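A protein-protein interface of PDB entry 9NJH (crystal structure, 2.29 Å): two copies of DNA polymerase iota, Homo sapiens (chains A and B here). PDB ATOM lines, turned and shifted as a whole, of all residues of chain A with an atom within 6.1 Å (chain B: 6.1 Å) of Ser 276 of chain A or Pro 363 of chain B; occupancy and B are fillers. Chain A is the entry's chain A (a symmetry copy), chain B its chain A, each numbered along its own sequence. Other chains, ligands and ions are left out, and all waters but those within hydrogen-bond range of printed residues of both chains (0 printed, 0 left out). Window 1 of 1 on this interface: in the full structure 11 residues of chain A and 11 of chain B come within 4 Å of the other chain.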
ATOM      1  N   LEU A 273      17.485 -33.597 -27.462  1.00  0.00           N
ATOM      2  CA  LEU A 273      16.757 -32.799 -28.484  1.00  0.00           C
ATOM      3  C   LEU A 273      17.072 -31.311 -28.329  1.00  0.00           C
ATOM      4  O   LEU A 273      16.834 -30.553 -29.281  1.00  0.00           O
ATOM      5  CB  LEU A 273      15.262 -33.068 -28.344  1.00  0.00           C
ATOM      6  CG  LEU A 273      14.679 -34.172 -29.231  1.00  0.00           C
ATOM      7  CD1 LEU A 273      14.984 -35.536 -28.646  1.00  0.00           C
ATOM      8  CD2 LEU A 273      13.182 -33.983 -29.359  1.00  0.00           C
ATOM      9  N   GLY A 274      17.580 -30.913 -27.174  1.00  0.00           N
ATOM     10  CA  GLY A 274      17.807 -29.481 -26.936  1.00  0.00           C
ATOM     11  C   GLY A 274      16.782 -28.952 -25.968  1.00  0.00           C
ATOM     12  O   GLY A 274      15.646 -29.441 -25.997  1.00  0.00           O
ATOM     13  N   ILE A 275      17.162 -27.969 -25.159  1.00  0.00           N
ATOM     14  CA  ILE A 275      16.245 -27.414 -24.125  1.00  0.00           C
ATOM     15  C   ILE A 275      15.020 -26.785 -24.806  1.00  0.00           C
ATOM     16  O   ILE A 275      13.913 -26.952 -24.276  1.00  0.00           O
ATOM     17  CB  ILE A 275      17.003 -26.412 -23.234  1.00  0.00           C
ATOM     18  CG1 ILE A 275      16.059 -25.615 -22.343  1.00  0.00           C
ATOM     19  CG2 ILE A 275      17.894 -25.502 -24.076  1.00  0.00           C
ATOM     20  CD1 ILE A 275      16.558 -25.438 -20.923  1.00  0.00           C
ATOM     21  N   SER A 276      15.208 -26.100 -25.932  1.00  0.00           N
ATOM     22  CA  SER A 276      14.072 -25.391 -26.576  1.00  0.00           C
ATOM     23  C   SER A 276      13.036 -26.398 -27.072  1.00  0.00           C
ATOM     24  O   SER A 276      11.884 -26.348 -26.601  1.00  0.00           O
ATOM     25  CB  SER A 276      14.547 -24.531 -27.711  1.00  0.00           C
ATOM     26  OG  SER A 276      13.485 -23.751 -28.239  1.00  0.00           O
ATOM     27  N   VAL A 277      13.454 -27.289 -27.961  1.00  0.00           N
ATOM     28  CA  VAL A 277      12.488 -28.245 -28.570  1.00  0.00           C
ATOM     29  C   VAL A 277      11.843 -29.081 -27.459  1.00  0.00           C
ATOM     30  O   VAL A 277      10.612 -29.166 -27.438  1.00  0.00           O
ATOM     31  CB  VAL A 277      13.192 -29.133 -29.611  1.00  0.00           C
ATOM     32  CG1 VAL A 277      12.381 -30.382 -29.933  1.00  0.00           C
ATOM     33  CG2 VAL A 277      13.523 -28.363 -30.881  1.00  0.00           C
ATOM     34  N   ALA A 278      12.646 -29.608 -26.542  1.00  0.00           N
ATOM     35  CA  ALA A 278      12.099 -30.519 -25.514  1.00  0.00           C
ATOM     36  C   ALA A 278      10.992 -29.835 -24.715  1.00  0.00           C
ATOM     37  O   ALA A 278       9.901 -30.414 -24.581  1.00  0.00           O
ATOM     38  CB  ALA A 278      13.219 -30.987 -24.633  1.00  0.00           C
ATOM     39  N   GLN A 279      11.247 -28.626 -24.238  1.00  0.00           N
ATOM     40  CA  GLN A 279      10.251 -27.953 -23.371  1.00  0.00           C
ATOM     41  C   GLN A 279       8.976 -27.677 -24.178  1.00  0.00           C
ATOM     42  O   GLN A 279       7.885 -28.010 -23.688  1.00  0.00           O
ATOM     43  CB  GLN A 279      10.886 -26.694 -22.786  1.00  0.00           C
ATOM     44  CG  GLN A 279      11.978 -26.981 -21.764  1.00  0.00           C
ATOM     45  CD  GLN A 279      12.398 -25.763 -20.967  1.00  0.00           C
ATOM     46  OE1 GLN A 279      12.065 -24.623 -21.306  1.00  0.00           O
ATOM     47  NE2 GLN A 279      13.135 -25.995 -19.892  1.00  0.00           N
ATOM     48  N   ARG A 280       9.126 -27.147 -25.390  1.00  0.00           N
ATOM     49  CA  ARG A 280       7.944 -26.801 -26.219  1.00  0.00           C
ATOM     50  C   ARG A 280       7.159 -28.067 -26.592  1.00  0.00           C
ATOM     51  O   ARG A 280       5.929 -28.040 -26.456  1.00  0.00           O
ATOM     52  CB  ARG A 280       8.384 -26.034 -27.470  1.00  0.00           C
ATOM     53  CG  ARG A 280       7.258 -25.502 -28.341  1.00  0.00           C
ATOM     54  CD  ARG A 280       7.800 -25.004 -29.666  1.00  0.00           C
ATOM     55  NE  ARG A 280       9.253 -24.809 -29.619  1.00  0.00           N
ATOM     56  CZ  ARG A 280      10.118 -25.438 -30.401  1.00  0.00           C
ATOM     57  NH1 ARG A 280       9.687 -26.289 -31.313  1.00  0.00           N
ATOM     58  NH2 ARG A 280      11.412 -25.214 -30.268  1.00  0.00           N
ATOM     59  N   ILE A 281       7.838 -29.137 -27.008  1.00  0.00           N
ATOM     60  CA  ILE A 281       7.110 -30.349 -27.492  1.00  0.00           C
ATOM     61  C   ILE A 281       6.400 -31.056 -26.325  1.00  0.00           C
ATOM     62  O   ILE A 281       5.305 -31.596 -26.541  1.00  0.00           O
ATOM     63  CB  ILE A 281       8.036 -31.296 -28.281  1.00  0.00           C
ATOM     64  CG1 ILE A 281       9.072 -31.977 -27.397  1.00  0.00           C
ATOM     65  CG2 ILE A 281       8.682 -30.569 -29.459  1.00  0.00           C
ATOM     66  CD1 ILE A 281       9.871 -33.048 -28.113  1.00  0.00           C
ATOM     67  N   HIS B 340      12.417 -12.648 -24.427  1.00  0.00           N
ATOM     68  CA  HIS B 340      11.773 -13.960 -24.699  1.00  0.00           C
ATOM     69  C   HIS B 340      12.830 -15.006 -25.056  1.00  0.00           C
ATOM     70  O   HIS B 340      12.494 -16.203 -25.082  1.00  0.00           O
ATOM     71  CB  HIS B 340      10.731 -13.835 -25.812  1.00  0.00           C
ATOM     72  CG  HIS B 340       9.441 -13.230 -25.372  1.00  0.00           C
ATOM     73  ND1 HIS B 340       8.228 -13.864 -25.515  1.00  0.00           N
ATOM     74  CD2 HIS B 340       9.174 -12.056 -24.795  1.00  0.00           C
ATOM     75  CE1 HIS B 340       7.271 -13.088 -25.035  1.00  0.00           C
ATOM     76  NE2 HIS B 340       7.824 -11.984 -24.591  1.00  0.00           N
ATOM     77  N   THR B 341      14.062 -14.578 -25.334  1.00  0.00           N
ATOM     78  CA  THR B 341      15.156 -15.534 -25.603  1.00  0.00           C
ATOM     79  C   THR B 341      16.377 -15.130 -24.806  1.00  0.00           C
ATOM     80  O   THR B 341      16.650 -13.922 -24.724  1.00  0.00           O
ATOM     81  CB  THR B 341      15.444 -15.603 -27.100  1.00  0.00           C
ATOM     82  OG1 THR B 341      14.191 -15.852 -27.724  1.00  0.00           O
ATOM     83  CG2 THR B 341      16.405 -16.720 -27.460  1.00  0.00           C
ATOM     84  N   VAL B 342      17.077 -16.102 -24.221  1.00  0.00           N
ATOM     85  CA  VAL B 342      18.310 -15.825 -23.427  1.00  0.00           C
ATOM     86  C   VAL B 342      19.492 -16.438 -24.177  1.00  0.00           C
ATOM     87  O   VAL B 342      19.298 -17.450 -24.862  1.00  0.00           O
ATOM     88  CB  VAL B 342      18.264 -16.363 -21.986  1.00  0.00           C
ATOM     89  CG1 VAL B 342      18.341 -17.883 -21.933  1.00  0.00           C
ATOM     90  CG2 VAL B 342      19.341 -15.738 -21.111  1.00  0.00           C
ATOM     91  N   GLN B 361      21.628 -20.339 -27.310  1.00  0.00           N
ATOM     92  CA  GLN B 361      20.441 -19.562 -26.882  1.00  0.00           C
ATOM     93  C   GLN B 361      19.252 -20.504 -26.645  1.00  0.00           C
ATOM     94  O   GLN B 361      19.270 -21.628 -27.173  1.00  0.00           O
ATOM     95  CB  GLN B 361      20.110 -18.490 -27.918  1.00  0.00           C
ATOM     96  CG  GLN B 361      19.472 -19.016 -29.197  1.00  0.00           C
ATOM     97  CD  GLN B 361      19.554 -18.027 -30.339  1.00  0.00           C
ATOM     98  OE1 GLN B 361      20.507 -17.251 -30.451  1.00  0.00           O
ATOM     99  NE2 GLN B 361      18.547 -18.043 -31.199  1.00  0.00           N
ATOM    100  N   CYS B 362      18.280 -20.054 -25.856  1.00  0.00           N
ATOM    101  CA  CYS B 362      17.076 -20.865 -25.565  1.00  0.00           C
ATOM    102  C   CYS B 362      15.912 -19.916 -25.283  1.00  0.00           C
ATOM    103  O   CYS B 362      16.123 -18.920 -24.574  1.00  0.00           O
ATOM    104  CB  CYS B 362      17.290 -21.760 -24.355  1.00  0.00           C
ATOM    105  SG  CYS B 362      15.973 -21.648 -23.120  1.00  0.00           S
ATOM    106  N   PRO B 363      14.703 -20.180 -25.812  1.00  0.00           N
ATOM    107  CA  PRO B 363      13.555 -19.349 -25.494  1.00  0.00           C
ATOM    108  C   PRO B 363      13.282 -19.404 -24.013  1.00  0.00           C
ATOM    109  O   PRO B 363      13.300 -20.493 -23.428  1.00  0.00           O
ATOM    110  CB  PRO B 363      12.449 -19.994 -26.311  1.00  0.00           C
ATOM    111  CG  PRO B 363      13.180 -20.715 -27.417  1.00  0.00           C
ATOM    112  CD  PRO B 363      14.421 -21.251 -26.740  1.00  0.00           C
ATOM    113  N   ILE B 364      13.032 -18.248 -23.412  1.00  0.00           N
ATOM    114  CA  ILE B 364      12.818 -18.187 -21.938  1.00  0.00           C
ATOM    115  C   ILE B 364      11.437 -18.757 -21.605  1.00  0.00           C
ATOM    116  O   ILE B 364      10.459 -18.356 -22.261  1.00  0.00           O
ATOM    117  CB  ILE B 364      12.944 -16.741 -21.436  1.00  0.00           C
ATOM    118  CG1 ILE B 364      14.345 -16.184 -21.667  1.00  0.00           C
ATOM    119  CG2 ILE B 364      12.518 -16.638 -19.973  1.00  0.00           C
ATOM    120  CD1 ILE B 364      14.407 -14.669 -21.709  1.00  0.00           C
ATOM    121  N   PRO B 365      11.322 -19.680 -20.630  1.00  0.00           N
ATOM    122  CA  PRO B 365      10.019 -20.174 -20.216  1.00  0.00           C
ATOM    123  C   PRO B 365       9.086 -19.046 -19.806  1.00  0.00           C
ATOM    124  O   PRO B 365       9.523 -18.114 -19.114  1.00  0.00           O
ATOM    125  CB  PRO B 365      10.401 -21.086 -19.057  1.00  0.00           C
ATOM    126  CG  PRO B 365      11.781 -21.571 -19.411  1.00  0.00           C
ATOM    127  CD  PRO B 365      12.435 -20.320 -19.961  1.00  0.00           C
ATOM    128  N   ILE B 386      18.765 -22.681 -16.563  1.00  0.00           N
ATOM    129  CA  ILE B 386      18.747 -22.690 -18.055  1.00  0.00           C
ATOM    130  C   ILE B 386      20.134 -22.297 -18.574  1.00  0.00           C
ATOM    131  O   ILE B 386      20.662 -22.998 -19.456  1.00  0.00           O
ATOM    132  CB  ILE B 386      17.675 -21.720 -18.571  1.00  0.00           C
ATOM    133  CG1 ILE B 386      16.275 -22.143 -18.141  1.00  0.00           C
ATOM    134  CG2 ILE B 386      17.779 -21.554 -20.085  1.00  0.00           C
ATOM    135  CD1 ILE B 386      15.336 -20.983 -17.870  1.00  0.00           C
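Cys 362 of chain B touches Ile 275 of chain A.
Ser 276 of chain A touches Pro 363 of chain B.
OE1 of Gln 279 of chain A touches CG of Pro 365 of chain B, at 3.6 Å.
No position is printed for both chains.
The side-chain hydroxyl (OG) of Ser 276 of chain A lies within hydrogen-bond range of the guanidinium group (NH2) of Arg 280 of chain A, at 3.2 Å.
The backbone carbonyl oxygen of Val 342 of chain B sits at hydrogen-bond distance from the backbone NH of Cys 362 of chain B, at 3.0 Å.
Printed residues of chain A that touch a printed residue of chain B: Ile 275, Ser 276 and Gln 279.
Among the printed residues, 3 pairs touch across the chains.
Gly 274 of chain A touches none of the printed residues of chain B.
Printed residues of chain B within 4 Å of Ile 275 of chain A: Cys 362 (3.8 Å).
Ser 276 of chain A touches one residue of chain B.
Printed residues of chain B within 4 Å of Gln 279 of chain A: Pro 365 (3.6 Å).
Thr 341 of chain B touches none of the printed residues of chain A.
Of chain A, only Ser 276 (3.1 Å) comes within 4 Å of Pro 363 of chain B.
Printed residues of chain A within 4 Å of Pro 365 of chain B: Gln 279 (3.6 Å).
The nearest residue of chain B that does not touch Ser 276 of chain A is Cys 362 of chain B (4.9 Å).
The nearest residue of chain A that does not touch Pro 363 of chain B is Gln 279 of chain A (4.8 Å).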
